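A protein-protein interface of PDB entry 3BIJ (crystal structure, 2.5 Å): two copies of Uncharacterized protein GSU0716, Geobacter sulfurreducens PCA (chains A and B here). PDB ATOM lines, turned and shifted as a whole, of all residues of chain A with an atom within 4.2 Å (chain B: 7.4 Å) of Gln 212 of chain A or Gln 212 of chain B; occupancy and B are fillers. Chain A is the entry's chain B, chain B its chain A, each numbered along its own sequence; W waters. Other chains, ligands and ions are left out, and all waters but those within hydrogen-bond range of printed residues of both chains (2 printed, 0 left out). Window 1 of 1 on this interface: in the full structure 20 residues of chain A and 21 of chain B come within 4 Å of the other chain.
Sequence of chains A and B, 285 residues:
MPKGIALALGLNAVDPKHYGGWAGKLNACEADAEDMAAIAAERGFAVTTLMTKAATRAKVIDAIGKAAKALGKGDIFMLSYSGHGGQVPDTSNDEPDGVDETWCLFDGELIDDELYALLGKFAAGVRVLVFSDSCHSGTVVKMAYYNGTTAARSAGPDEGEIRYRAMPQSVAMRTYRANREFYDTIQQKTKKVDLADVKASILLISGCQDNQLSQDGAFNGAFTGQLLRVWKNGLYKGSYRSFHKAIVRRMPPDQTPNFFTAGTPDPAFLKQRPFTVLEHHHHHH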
ATOM      1  N   CYS A 135     -17.668 -28.243  14.305  1.00  0.00           N
ATOM      2  CA  CYS A 135     -18.792 -27.346  14.040  1.00  0.00           C
ATOM      3  C   CYS A 135     -20.090 -28.146  13.982  1.00  0.00           C
ATOM      4  O   CYS A 135     -20.088 -29.359  14.180  1.00  0.00           O
ATOM      5  CB  CYS A 135     -18.584 -26.636  12.705  1.00  0.00           C
ATOM      6  SG  CYS A 135     -18.561 -27.785  11.279  1.00  0.00           S
ATOM      7  N   LYS A 142     -27.945 -21.699   7.864  1.00  0.00           N
ATOM      8  CA  LYS A 142     -26.498 -21.859   7.760  1.00  0.00           C
ATOM      9  C   LYS A 142     -26.232 -22.594   6.472  1.00  0.00           C
ATOM     10  O   LYS A 142     -25.324 -22.256   5.713  1.00  0.00           O
ATOM     11  CB  LYS A 142     -25.935 -22.682   8.929  1.00  0.00           C
ATOM     12  CG  LYS A 142     -24.411 -22.791   8.910  1.00  0.00           C
ATOM     13  CD  LYS A 142     -23.845 -23.706   9.993  1.00  0.00           C
ATOM     14  CE  LYS A 142     -24.083 -23.171  11.384  1.00  0.00           C
ATOM     15  NZ  LYS A 142     -23.432 -23.994  12.435  1.00  0.00           N
ATOM     16  N   TYR A 146     -24.005 -21.303   3.186  1.00  0.00           N
ATOM     17  CA  TYR A 146     -22.893 -22.129   2.719  1.00  0.00           C
ATOM     18  C   TYR A 146     -23.184 -22.970   1.481  1.00  0.00           C
ATOM     19  O   TYR A 146     -22.278 -23.589   0.935  1.00  0.00           O
ATOM     20  CB  TYR A 146     -22.436 -23.087   3.824  1.00  0.00           C
ATOM     21  CG  TYR A 146     -21.495 -22.491   4.846  1.00  0.00           C
ATOM     22  CD1 TYR A 146     -20.193 -22.143   4.505  1.00  0.00           C
ATOM     23  CD2 TYR A 146     -21.913 -22.271   6.157  1.00  0.00           C
ATOM     24  CE1 TYR A 146     -19.335 -21.588   5.450  1.00  0.00           C
ATOM     25  CE2 TYR A 146     -21.065 -21.717   7.106  1.00  0.00           C
ATOM     26  CZ  TYR A 146     -19.784 -21.378   6.749  1.00  0.00           C
ATOM     27  OH  TYR A 146     -18.956 -20.812   7.682  1.00  0.00           O
ATOM     28  N   CYS A 208     -15.142 -22.325  15.628  1.00  0.00           N
ATOM     29  CA  CYS A 208     -15.980 -21.363  14.931  1.00  0.00           C
ATOM     30  C   CYS A 208     -17.203 -20.937  15.747  1.00  0.00           C
ATOM     31  O   CYS A 208     -17.443 -21.444  16.842  1.00  0.00           O
ATOM     32  CB  CYS A 208     -16.435 -21.958  13.594  1.00  0.00           C
ATOM     33  SG  CYS A 208     -17.580 -23.353  13.737  1.00  0.00           S
ATOM     34  N   GLN A 209     -17.959 -19.990  15.197  1.00  0.00           N
ATOM     35  CA  GLN A 209     -19.165 -19.473  15.829  1.00  0.00           C
ATOM     36  C   GLN A 209     -20.334 -20.413  15.505  1.00  0.00           C
ATOM     37  O   GLN A 209     -20.251 -21.222  14.575  1.00  0.00           O
ATOM     38  CB  GLN A 209     -19.507 -18.072  15.300  1.00  0.00           C
ATOM     39  CG  GLN A 209     -18.400 -17.040  15.422  1.00  0.00           C
ATOM     40  CD  GLN A 209     -18.051 -16.722  16.850  1.00  0.00           C
ATOM     41  OE1 GLN A 209     -16.893 -16.443  17.168  1.00  0.00           O
ATOM     42  NE2 GLN A 209     -19.050 -16.761  17.729  1.00  0.00           N
ATOM     43  N   ASP A 210     -21.422 -20.277  16.264  1.00  0.00           N
ATOM     44  CA  ASP A 210     -22.622 -21.097  16.102  1.00  0.00           C
ATOM     45  C   ASP A 210     -23.277 -20.954  14.744  1.00  0.00           C
ATOM     46  O   ASP A 210     -24.054 -21.816  14.329  1.00  0.00           O
ATOM     47  CB  ASP A 210     -23.644 -20.761  17.189  1.00  0.00           C
ATOM     48  CG  ASP A 210     -23.159 -21.118  18.562  1.00  0.00           C
ATOM     49  OD1 ASP A 210     -23.856 -20.793  19.552  1.00  0.00           O
ATOM     50  OD2 ASP A 210     -22.076 -21.735  18.651  1.00  0.00           O
ATOM     51  N   ASN A 211     -22.987 -19.856  14.058  1.00  0.00           N
ATOM     52  CA  ASN A 211     -23.556 -19.633  12.739  1.00  0.00           C
ATOM     53  C   ASN A 211     -22.517 -19.900  11.667  1.00  0.00           C
ATOM     54  O   ASN A 211     -22.711 -19.533  10.512  1.00  0.00           O
ATOM     55  CB  ASN A 211     -24.054 -18.195  12.583  1.00  0.00           C
ATOM     56  CG  ASN A 211     -22.929 -17.182  12.618  1.00  0.00           C
ATOM     57  OD1 ASN A 211     -23.065 -16.080  12.094  1.00  0.00           O
ATOM     58  ND2 ASN A 211     -21.815 -17.544  13.249  1.00  0.00           N
ATOM     59  N   GLN A 212     -21.405 -20.521  12.042  1.00  0.00           N
ATOM     60  CA  GLN A 212     -20.369 -20.824  11.063  1.00  0.00           C
ATOM     61  C   GLN A 212     -20.059 -22.319  11.054  1.00  0.00           C
ATOM     62  O   GLN A 212     -20.621 -23.092  11.835  1.00  0.00           O
ATOM     63  CB  GLN A 212     -19.094 -20.041  11.375  1.00  0.00           C
ATOM     64  CG  GLN A 212     -19.245 -18.531  11.307  1.00  0.00           C
ATOM     65  CD  GLN A 212     -17.994 -17.836  11.767  1.00  0.00           C
ATOM     66  OE1 GLN A 212     -17.386 -18.247  12.757  1.00  0.00           O
ATOM     67  NE2 GLN A 212     -17.592 -16.779  11.059  1.00  0.00           N
ATOM     68  N   LEU A 213     -19.169 -22.712  10.149  1.00  0.00           N
ATOM     69  CA  LEU A 213     -18.739 -24.090  10.035  1.00  0.00           C
ATOM     70  C   LEU A 213     -17.222 -24.105  10.163  1.00  0.00           C
ATOM     71  O   LEU A 213     -16.559 -23.111   9.848  1.00  0.00           O
ATOM     72  CB  LEU A 213     -19.138 -24.675   8.689  1.00  0.00           C
ATOM     73  CG  LEU A 213     -20.606 -25.004   8.462  1.00  0.00           C
ATOM     74  CD1 LEU A 213     -20.723 -25.664   7.103  1.00  0.00           C
ATOM     75  CD2 LEU A 213     -21.135 -25.937   9.553  1.00  0.00           C
ATOM     76  N   PRO A 253     -13.044 -14.473   7.726  1.00  0.00           N
ATOM     77  CA  PRO A 253     -14.297 -13.997   8.330  1.00  0.00           C
ATOM     78  C   PRO A 253     -15.439 -15.007   8.421  1.00  0.00           C
ATOM     79  O   PRO A 253     -16.334 -14.857   9.257  1.00  0.00           O
ATOM     80  CB  PRO A 253     -14.652 -12.775   7.481  1.00  0.00           C
ATOM     81  CG  PRO A 253     -14.073 -13.113   6.147  1.00  0.00           C
ATOM     82  CD  PRO A 253     -12.721 -13.710   6.510  1.00  0.00           C
ATOM     83  N   ASP A 254     -15.387 -16.044   7.586  1.00  0.00           N
ATOM     84  CA  ASP A 254     -16.416 -17.076   7.574  1.00  0.00           C
ATOM     85  C   ASP A 254     -16.149 -18.177   8.611  1.00  0.00           C
ATOM     86  O   ASP A 254     -16.928 -19.127   8.744  1.00  0.00           O
ATOM     87  CB  ASP A 254     -16.533 -17.686   6.172  1.00  0.00           C
ATOM     88  CG  ASP A 254     -15.394 -18.621   5.848  1.00  0.00           C
ATOM     89  OD1 ASP A 254     -14.220 -18.217   6.015  1.00  0.00           O
ATOM     90  OD2 ASP A 254     -15.669 -19.770   5.423  1.00  0.00           O
ATOM     91  N   GLN A 255     -15.028 -18.053   9.320  1.00  0.00           N
ATOM     92  CA  GLN A 255     -14.665 -18.993  10.377  1.00  0.00           C
ATOM     93  C   GLN A 255     -13.900 -18.269  11.475  1.00  0.00           C
ATOM     94  O   GLN A 255     -12.714 -17.967  11.323  1.00  0.00           O
ATOM     95  CB  GLN A 255     -13.799 -20.147   9.866  1.00  0.00           C
ATOM     96  CG  GLN A 255     -13.759 -21.277  10.884  1.00  0.00           C
ATOM     97  CD  GLN A 255     -12.900 -22.473  10.481  1.00  0.00           C
ATOM     98  OE1 GLN A 255     -12.703 -22.762   9.303  1.00  0.00           O
ATOM     99  NE2 GLN A 255     -12.406 -23.187  11.479  1.00  0.00           N
ATOM    100  N   THR A 256     -14.587 -17.987  12.582  1.00  0.00           N
ATOM    101  CA  THR A 256     -13.974 -17.299  13.707  1.00  0.00           C
ATOM    102  C   THR A 256     -14.048 -18.150  14.965  1.00  0.00           C
ATOM    103  O   THR A 256     -15.130 -18.451  15.436  1.00  0.00           O
ATOM    104  CB  THR A 256     -14.686 -15.956  14.021  1.00  0.00           C
ATOM    105  OG1 THR A 256     -14.847 -15.208  12.814  1.00  0.00           O
ATOM    106  CG2 THR A 256     -13.857 -15.126  15.003  1.00  0.00           C
ATOM    107  N   SER B 134     -21.188  -1.868  14.886  1.00  0.00           N
ATOM    108  CA  SER B 134     -20.082  -1.253  14.172  1.00  0.00           C
ATOM    109  C   SER B 134     -18.967  -2.293  14.003  1.00  0.00           C
ATOM    110  O   SER B 134     -19.102  -3.433  14.446  1.00  0.00           O
ATOM    111  CB  SER B 134     -19.579  -0.056  14.984  1.00  0.00           C
ATOM    112  OG  SER B 134     -18.572   0.651  14.305  1.00  0.00           O
ATOM    113  N   CYS B 135     -17.868  -1.887  13.371  1.00  0.00           N
ATOM    114  CA  CYS B 135     -16.737  -2.778  13.139  1.00  0.00           C
ATOM    115  C   CYS B 135     -15.457  -1.969  12.973  1.00  0.00           C
ATOM    116  O   CYS B 135     -15.476  -0.742  13.066  1.00  0.00           O
ATOM    117  CB  CYS B 135     -16.982  -3.599  11.881  1.00  0.00           C
ATOM    118  SG  CYS B 135     -17.082  -2.581  10.410  1.00  0.00           S
ATOM    119  N   HIS B 136     -14.348  -2.660  12.719  1.00  0.00           N
ATOM    120  CA  HIS B 136     -13.055  -1.999  12.544  1.00  0.00           C
ATOM    121  C   HIS B 136     -12.321  -2.559  11.339  1.00  0.00           C
ATOM    122  O   HIS B 136     -12.488  -3.726  11.005  1.00  0.00           O
ATOM    123  CB  HIS B 136     -12.207  -2.184  13.801  1.00  0.00           C
ATOM    124  CG  HIS B 136     -12.771  -1.490  15.000  1.00  0.00           C
ATOM    125  ND1 HIS B 136     -12.724  -0.121  15.157  1.00  0.00           N
ATOM    126  CD2 HIS B 136     -13.450  -1.969  16.071  1.00  0.00           C
ATOM    127  CE1 HIS B 136     -13.350   0.214  16.272  1.00  0.00           C
ATOM    128  NE2 HIS B 136     -13.801  -0.888  16.845  1.00  0.00           N
ATOM    129  N   SER B 137     -11.520  -1.730  10.677  1.00  0.00           N
ATOM    130  CA  SER B 137     -10.763  -2.188   9.516  1.00  0.00           C
ATOM    131  C   SER B 137      -9.871  -3.354   9.901  1.00  0.00           C
ATOM    132  O   SER B 137      -9.588  -4.218   9.081  1.00  0.00           O
ATOM    133  CB  SER B 137      -9.881  -1.070   8.969  1.00  0.00           C
ATOM    134  OG  SER B 137     -10.658  -0.027   8.430  1.00  0.00           O
ATOM    135  N   GLY B 138      -9.429  -3.375  11.153  1.00  0.00           N
ATOM    136  CA  GLY B 138      -8.548  -4.439  11.592  1.00  0.00           C
ATOM    137  C   GLY B 138      -7.221  -4.351  10.854  1.00  0.00           C
ATOM    138  O   GLY B 138      -6.731  -3.256  10.545  1.00  0.00           O
ATOM    139  N   LYS B 142      -7.696  -8.811   7.176  1.00  0.00           N
ATOM    140  CA  LYS B 142      -9.143  -8.673   7.103  1.00  0.00           C
ATOM    141  C   LYS B 142      -9.462  -8.046   5.768  1.00  0.00           C
ATOM    142  O   LYS B 142     -10.392  -8.457   5.073  1.00  0.00           O
ATOM    143  CB  LYS B 142      -9.677  -7.768   8.223  1.00  0.00           C
ATOM    144  CG  LYS B 142     -11.201  -7.671   8.237  1.00  0.00           C
ATOM    145  CD  LYS B 142     -11.733  -6.677   9.255  1.00  0.00           C
ATOM    146  CE  LYS B 142     -11.444  -7.100  10.677  1.00  0.00           C
ATOM    147  NZ  LYS B 142     -12.095  -6.201  11.682  1.00  0.00           N
ATOM    148  N   TYR B 146     -11.747  -9.634   2.678  1.00  0.00           N
ATOM    149  CA  TYR B 146     -12.883  -8.869   2.178  1.00  0.00           C
ATOM    150  C   TYR B 146     -12.679  -8.230   0.807  1.00  0.00           C
ATOM    151  O   TYR B 146     -13.510  -7.438   0.361  1.00  0.00           O
ATOM    152  CB  TYR B 146     -13.311  -7.805   3.197  1.00  0.00           C
ATOM    153  CG  TYR B 146     -14.223  -8.321   4.296  1.00  0.00           C
ATOM    154  CD1 TYR B 146     -15.538  -8.700   4.025  1.00  0.00           C
ATOM    155  CD2 TYR B 146     -13.763  -8.444   5.607  1.00  0.00           C
ATOM    156  CE1 TYR B 146     -16.374  -9.193   5.041  1.00  0.00           C
ATOM    157  CE2 TYR B 146     -14.589  -8.934   6.625  1.00  0.00           C
ATOM    158  CZ  TYR B 146     -15.889  -9.309   6.336  1.00  0.00           C
ATOM    159  OH  TYR B 146     -16.691  -9.803   7.345  1.00  0.00           O
ATOM    160  N   TYR B 164     -19.939  -1.031   4.742  1.00  0.00           N
ATOM    161  CA  TYR B 164     -19.548  -1.558   6.030  1.00  0.00           C
ATOM    162  C   TYR B 164     -19.253  -0.376   6.950  1.00  0.00           C
ATOM    163  O   TYR B 164     -18.740   0.651   6.515  1.00  0.00           O
ATOM    164  CB  TYR B 164     -18.322  -2.447   5.855  1.00  0.00           C
ATOM    165  CG  TYR B 164     -18.606  -3.740   5.119  1.00  0.00           C
ATOM    166  CD1 TYR B 164     -19.303  -4.778   5.744  1.00  0.00           C
ATOM    167  CD2 TYR B 164     -18.133  -3.953   3.825  1.00  0.00           C
ATOM    168  CE1 TYR B 164     -19.511  -6.001   5.106  1.00  0.00           C
ATOM    169  CE2 TYR B 164     -18.336  -5.175   3.171  1.00  0.00           C
ATOM    170  CZ  TYR B 164     -19.020  -6.189   3.821  1.00  0.00           C
ATOM    171  OH  TYR B 164     -19.187  -7.414   3.228  1.00  0.00           O
ATOM    172  N   ALA B 166     -17.013   0.630   8.859  1.00  0.00           N
ATOM    173  CA  ALA B 166     -15.619   0.749   9.263  1.00  0.00           C
ATOM    174  C   ALA B 166     -14.966   1.842   8.432  1.00  0.00           C
ATOM    175  O   ALA B 166     -15.142   1.905   7.212  1.00  0.00           O
ATOM    176  CB  ALA B 166     -14.893  -0.567   9.047  1.00  0.00           C
ATOM    177  N   GLY B 207     -21.853  -5.973  16.766  1.00  0.00           N
ATOM    178  CA  GLY B 207     -22.398  -6.479  15.519  1.00  0.00           C
ATOM    179  C   GLY B 207     -21.595  -7.557  14.813  1.00  0.00           C
ATOM    180  O   GLY B 207     -22.123  -8.301  13.982  1.00  0.00           O
ATOM    181  N   CYS B 208     -20.311  -7.657  15.123  1.00  0.00           N
ATOM    182  CA  CYS B 208     -19.493  -8.670  14.465  1.00  0.00           C
ATOM    183  C   CYS B 208     -18.244  -9.043  15.265  1.00  0.00           C
ATOM    184  O   CYS B 208     -17.971  -8.464  16.316  1.00  0.00           O
ATOM    185  CB  CYS B 208     -19.085  -8.167  13.075  1.00  0.00           C
ATOM    186  SG  CYS B 208     -17.947  -6.750  13.099  1.00  0.00           S
ATOM    187  N   GLN B 209     -17.493 -10.016  14.745  1.00  0.00           N
ATOM    188  CA  GLN B 209     -16.258 -10.486  15.370  1.00  0.00           C
ATOM    189  C   GLN B 209     -15.112  -9.566  14.941  1.00  0.00           C
ATOM    190  O   GLN B 209     -15.236  -8.820  13.961  1.00  0.00           O
ATOM    191  CB  GLN B 209     -15.930 -11.919  14.933  1.00  0.00           C
ATOM    192  CG  GLN B 209     -17.027 -12.938  15.186  1.00  0.00           C
ATOM    193  CD  GLN B 209     -17.321 -13.145  16.648  1.00  0.00           C
ATOM    194  OE1 GLN B 209     -18.454 -13.420  17.016  1.00  0.00           O
ATOM    195  NE2 GLN B 209     -16.299 -13.037  17.491  1.00  0.00           N
ATOM    196  N   ASP B 210     -13.998  -9.638  15.671  1.00  0.00           N
ATOM    197  CA  ASP B 210     -12.818  -8.822  15.398  1.00  0.00           C
ATOM    198  C   ASP B 210     -12.208  -9.062  14.014  1.00  0.00           C
ATOM    199  O   ASP B 210     -11.456  -8.230  13.494  1.00  0.00           O
ATOM    200  CB  ASP B 210     -11.755  -9.066  16.471  1.00  0.00           C
ATOM    201  CG  ASP B 210     -12.203  -8.620  17.835  1.00  0.00           C
ATOM    202  OD1 ASP B 210     -11.476  -8.877  18.825  1.00  0.00           O
ATOM    203  OD2 ASP B 210     -13.290  -8.003  17.919  1.00  0.00           O
ATOM    204  N   ASN B 211     -12.514 -10.210  13.425  1.00  0.00           N
ATOM    205  CA  ASN B 211     -12.001 -10.518  12.103  1.00  0.00           C
ATOM    206  C   ASN B 211     -13.086 -10.318  11.057  1.00  0.00           C
ATOM    207  O   ASN B 211     -12.935 -10.731   9.911  1.00  0.00           O
ATOM    208  CB  ASN B 211     -11.496 -11.961  12.026  1.00  0.00           C
ATOM    209  CG  ASN B 211     -12.604 -12.981  12.207  1.00  0.00           C
ATOM    210  OD1 ASN B 211     -12.476 -14.123  11.768  1.00  0.00           O
ATOM    211  ND2 ASN B 211     -13.691 -12.580  12.865  1.00  0.00           N
ATOM    212  N   GLN B 212     -14.194  -9.696  11.447  1.00  0.00           N
ATOM    213  CA  GLN B 212     -15.275  -9.470  10.491  1.00  0.00           C
ATOM    214  C   GLN B 212     -15.595  -7.989  10.365  1.00  0.00           C
ATOM    215  O   GLN B 212     -14.973  -7.156  11.016  1.00  0.00           O
ATOM    216  CB  GLN B 212     -16.533 -10.235  10.908  1.00  0.00           C
ATOM    217  CG  GLN B 212     -16.349 -11.738  10.983  1.00  0.00           C
ATOM    218  CD  GLN B 212     -17.572 -12.419  11.523  1.00  0.00           C
ATOM    219  OE1 GLN B 212     -18.148 -11.964  12.510  1.00  0.00           O
ATOM    220  NE2 GLN B 212     -17.985 -13.515  10.886  1.00  0.00           N
ATOM    221  N   LEU B 213     -16.554  -7.674   9.502  1.00  0.00           N
ATOM    222  CA  LEU B 213     -16.986  -6.299   9.296  1.00  0.00           C
ATOM    223  C   LEU B 213     -18.486  -6.277   9.466  1.00  0.00           C
ATOM    224  O   LEU B 213     -19.152  -7.282   9.202  1.00  0.00           O
ATOM    225  CB  LEU B 213     -16.639  -5.815   7.892  1.00  0.00           C
ATOM    226  CG  LEU B 213     -15.182  -5.491   7.578  1.00  0.00           C
ATOM    227  CD1 LEU B 213     -15.129  -4.932   6.181  1.00  0.00           C
ATOM    228  CD2 LEU B 213     -14.618  -4.477   8.581  1.00  0.00           C
ATOM    229  N   SER B 214     -19.014  -5.138   9.908  1.00  0.00           N
ATOM    230  CA  SER B 214     -20.455  -4.982  10.118  1.00  0.00           C
ATOM    231  C   SER B 214     -21.097  -4.272   8.946  1.00  0.00           C
ATOM    232  O   SER B 214     -20.679  -3.184   8.560  1.00  0.00           O
ATOM    233  CB  SER B 214     -20.736  -4.202  11.404  1.00  0.00           C
ATOM    234  OG  SER B 214     -20.480  -5.004  12.534  1.00  0.00           O
ATOM    235  N   VAL B 248     -27.633 -14.499  16.131  1.00  0.00           N
ATOM    236  CA  VAL B 248     -26.558 -15.078  15.340  1.00  0.00           C
ATOM    237  C   VAL B 248     -27.068 -16.187  14.422  1.00  0.00           C
ATOM    238  O   VAL B 248     -26.561 -16.368  13.324  1.00  0.00           O
ATOM    239  CB  VAL B 248     -25.416 -15.641  16.224  1.00  0.00           C
ATOM    240  CG1 VAL B 248     -24.978 -14.596  17.230  1.00  0.00           C
ATOM    241  CG2 VAL B 248     -25.851 -16.908  16.904  1.00  0.00           C
ATOM    242  N   MET B 251     -28.031 -14.551  11.256  1.00  0.00           N
ATOM    243  CA  MET B 251     -26.947 -13.804  10.640  1.00  0.00           C
ATOM    244  C   MET B 251     -26.068 -14.626   9.717  1.00  0.00           C
ATOM    245  O   MET B 251     -25.847 -15.806   9.946  1.00  0.00           O
ATOM    246  CB  MET B 251     -26.072 -13.219  11.734  1.00  0.00           C
ATOM    247  CG  MET B 251     -26.777 -12.218  12.629  1.00  0.00           C
ATOM    248  SD  MET B 251     -27.181 -10.555  11.682  1.00  0.00           S
ATOM    249  CE  MET B 251     -25.407  -9.784  11.627  1.00  0.00           C
ATOM    250  N   PRO B 252     -25.532 -13.997   8.665  1.00  0.00           N
ATOM    251  CA  PRO B 252     -24.661 -14.685   7.712  1.00  0.00           C
ATOM    252  C   PRO B 252     -23.323 -15.026   8.384  1.00  0.00           C
ATOM    253  O   PRO B 252     -22.871 -14.316   9.294  1.00  0.00           O
ATOM    254  CB  PRO B 252     -24.516 -13.667   6.587  1.00  0.00           C
ATOM    255  CG  PRO B 252     -24.612 -12.342   7.304  1.00  0.00           C
ATOM    256  CD  PRO B 252     -25.736 -12.588   8.282  1.00  0.00           C
ATOM    257  N   PRO B 253     -22.662 -16.111   7.940  1.00  0.00           N
ATOM    258  CA  PRO B 253     -21.382 -16.533   8.521  1.00  0.00           C
ATOM    259  C   PRO B 253     -20.249 -15.512   8.485  1.00  0.00           C
ATOM    260  O   PRO B 253     -19.310 -15.619   9.268  1.00  0.00           O
ATOM    261  CB  PRO B 253     -21.055 -17.808   7.749  1.00  0.00           C
ATOM    262  CG  PRO B 253     -21.693 -17.567   6.410  1.00  0.00           C
ATOM    263  CD  PRO B 253     -23.030 -16.960   6.794  1.00  0.00           C
ATOM    264  N   ASP B 254     -20.349 -14.522   7.594  1.00  0.00           N
ATOM    265  CA  ASP B 254     -19.316 -13.492   7.461  1.00  0.00           C
ATOM    266  C   ASP B 254     -19.559 -12.322   8.428  1.00  0.00           C
ATOM    267  O   ASP B 254     -18.776 -11.365   8.481  1.00  0.00           O
ATOM    268  CB  ASP B 254     -19.256 -12.986   6.012  1.00  0.00           C
ATOM    269  CG  ASP B 254     -20.421 -12.096   5.656  1.00  0.00           C
ATOM    270  OD1 ASP B 254     -21.588 -12.494   5.874  1.00  0.00           O
ATOM    271  OD2 ASP B 254     -20.172 -10.984   5.144  1.00  0.00           O
ATOM    272  N   GLN B 255     -20.661 -12.397   9.173  1.00  0.00           N
ATOM    273  CA  GLN B 255     -21.001 -11.384  10.170  1.00  0.00           C
ATOM    274  C   GLN B 255     -21.705 -12.027  11.364  1.00  0.00           C
ATOM    275  O   GLN B 255     -22.891 -12.348  11.298  1.00  0.00           O
ATOM    276  CB  GLN B 255     -21.911 -10.284   9.605  1.00  0.00           C
ATOM    277  CG  GLN B 255     -21.918  -9.084  10.550  1.00  0.00           C
ATOM    278  CD  GLN B 255     -22.781  -7.915  10.108  1.00  0.00           C
ATOM    279  OE1 GLN B 255     -23.007  -7.697   8.925  1.00  0.00           O
ATOM    280  NE2 GLN B 255     -23.238  -7.139  11.070  1.00  0.00           N
ATOM    281  N   THR B 256     -20.970 -12.209  12.456  1.00  0.00           N
ATOM    282  CA  THR B 256     -21.526 -12.833  13.652  1.00  0.00           C
ATOM    283  C   THR B 256     -21.392 -11.903  14.842  1.00  0.00           C
ATOM    284  O   THR B 256     -20.278 -11.577  15.248  1.00  0.00           O
ATOM    285  CB  THR B 256     -20.788 -14.151  14.015  1.00  0.00           C
ATOM    286  OG1 THR B 256     -20.713 -14.999  12.865  1.00  0.00           O
ATOM    287  CG2 THR B 256     -21.530 -14.885  15.130  1.00  0.00           C
ATOM    288  N   PRO B 257     -22.524 -11.444  15.404  1.00  0.00           N
ATOM    289  CA  PRO B 257     -22.421 -10.551  16.561  1.00  0.00           C
ATOM    290  C   PRO B 257     -21.792 -11.308  17.722  1.00  0.00           C
ATOM    291  O   PRO B 257     -21.964 -12.524  17.851  1.00  0.00           O
ATOM    292  CB  PRO B 257     -23.873 -10.119  16.806  1.00  0.00           C
ATOM    293  CG  PRO B 257     -24.692 -11.193  16.151  1.00  0.00           C
ATOM    294  CD  PRO B 257     -23.910 -11.501  14.906  1.00  0.00           C
ATOM    295  N   ASN B 258     -21.044 -10.584  18.547  1.00  0.00           N
ATOM    296  CA  ASN B 258     -20.353 -11.178  19.679  1.00  0.00           C
ATOM    297  C   ASN B 258     -20.992 -10.883  21.035  1.00  0.00           C
ATOM    298  O   ASN B 258     -21.587  -9.825  21.255  1.00  0.00           O
ATOM    299  CB  ASN B 258     -18.913 -10.691  19.695  1.00  0.00           C
ATOM    300  CG  ASN B 258     -17.999 -11.616  20.449  1.00  0.00           C
ATOM    301  OD1 ASN B 258     -17.088 -11.165  21.135  1.00  0.00           O
ATOM    302  ND2 ASN B 258     -18.228 -12.923  20.322  1.00  0.00           N
HETATM  303  O   HOH W   1     -25.488 -18.739   9.195  1.00  0.00           O
HETATM  304  O   HOH W   2     -20.623 -14.913  18.935  1.00  0.00           O
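Asn 211 of chain A touches Thr 256 of chain B, and with the chains exchanged Thr 256 of chain A touches Asn 211 of chain B. Of the 20 pairs that touch across the chains among the printed residues, 17 have their exchanged pair printed and touching as well.
OE1 of Gln 209 of chain B is in hydrogen-bond range of ND2 of Asn 258 of chain B, 3.4 Å away. The side-chain amide oxygen (OE1) of Gln 212 of chain A lies within hydrogen-bond range of the backbone NH (N) of Thr 256 of chain A (2.8 Å).
Among the printed residues, pairs that only touch across the chains: Asn 211 of chain A with Val 248 of chain B (3.2 Å), Asn 211 of chain A with Met 251 of chain B (3.5 Å), Pro 253 of chain A with Tyr 146 of chain B (3.6 Å), Pro 253 of chain A with Asn 211 of chain B (3.6 Å), Asn 211 of chain A with Pro 253 of chain B (3.7 Å), Asp 254 of chain A with Pro 253 of chain B (3.7 Å), Tyr 146 of chain A with Pro 253 of chain B (3.7 Å), Pro 253 of chain A with Asp 254 of chain B (3.7 Å), Gln 209 of chain A with Thr 256 of chain B (3.8 Å), Thr 256 of chain A with Gln 209 of chain B (3.8 Å), Asn 211 of chain A with Gln 255 of chain B (3.8 Å) and Gln 255 of chain A with Asn 211 of chain B (3.9 Å).
Gln 212 of chain A touches two residues of chain B. Of the printed residues of chain A, Asn 211 of chain B touches Pro 253 (3.6 Å), Gln 255 (3.9 Å) and Thr 256 (2.8 Å). Printed residues of chain B within 4 Å of Gln 255 of chain A: Asn 211 (3.9 Å). The nearest residue of chain B that does not touch Gln 212 of chain A is Thr 256 of chain B (4.02 Å). The nearest residue of chain A that does not touch Gln 212 of chain B is Thr 256 of chain A (4.1 Å).
OE1 of Gln 209 of chain B sits close to OE1 of Gln 209 of chain A (3.4 Å). The side-chain amide oxygen of Asn 211 of chain B lies within hydrogen-bond range of the side-chain hydroxyl of Thr 256 of chain A. NE2 of Gln 212 of chain B lies close to NE2 of Gln 212 of chain A (3.3 Å). The backbone carbonyl oxygen (O) of Pro 253 of chain A lies within hydrogen-bond range of the side-chain amide nitrogen (NE2) of Gln 212 of chain B, 2.7 Å away. OD1 of Asn 211 of chain A lies close to O of Pro 252 of chain B (3.3 Å). O of Pro 253 of chain B sits at hydrogen-bond distance from NE2 of Gln 212 of chain A, 2.7 Å away. The side-chain hydroxyl (OG1) of Thr 256 of chain B sits at hydrogen-bond distance from the side-chain amide oxygen (OD1) of Asn 211 of chain A. The backbone carbonyl oxygen of Pro 253 of chain B sits close to the backbone carbonyl oxygen of Pro 253 of chain A, at 3.1 Å.
Among the printed residues, 20 pairs touch across the chains. Among the printed residues, no Asp or Glu carboxylate lies within 4 Å of a Lys or Arg side-chain nitrogen of the other chain.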
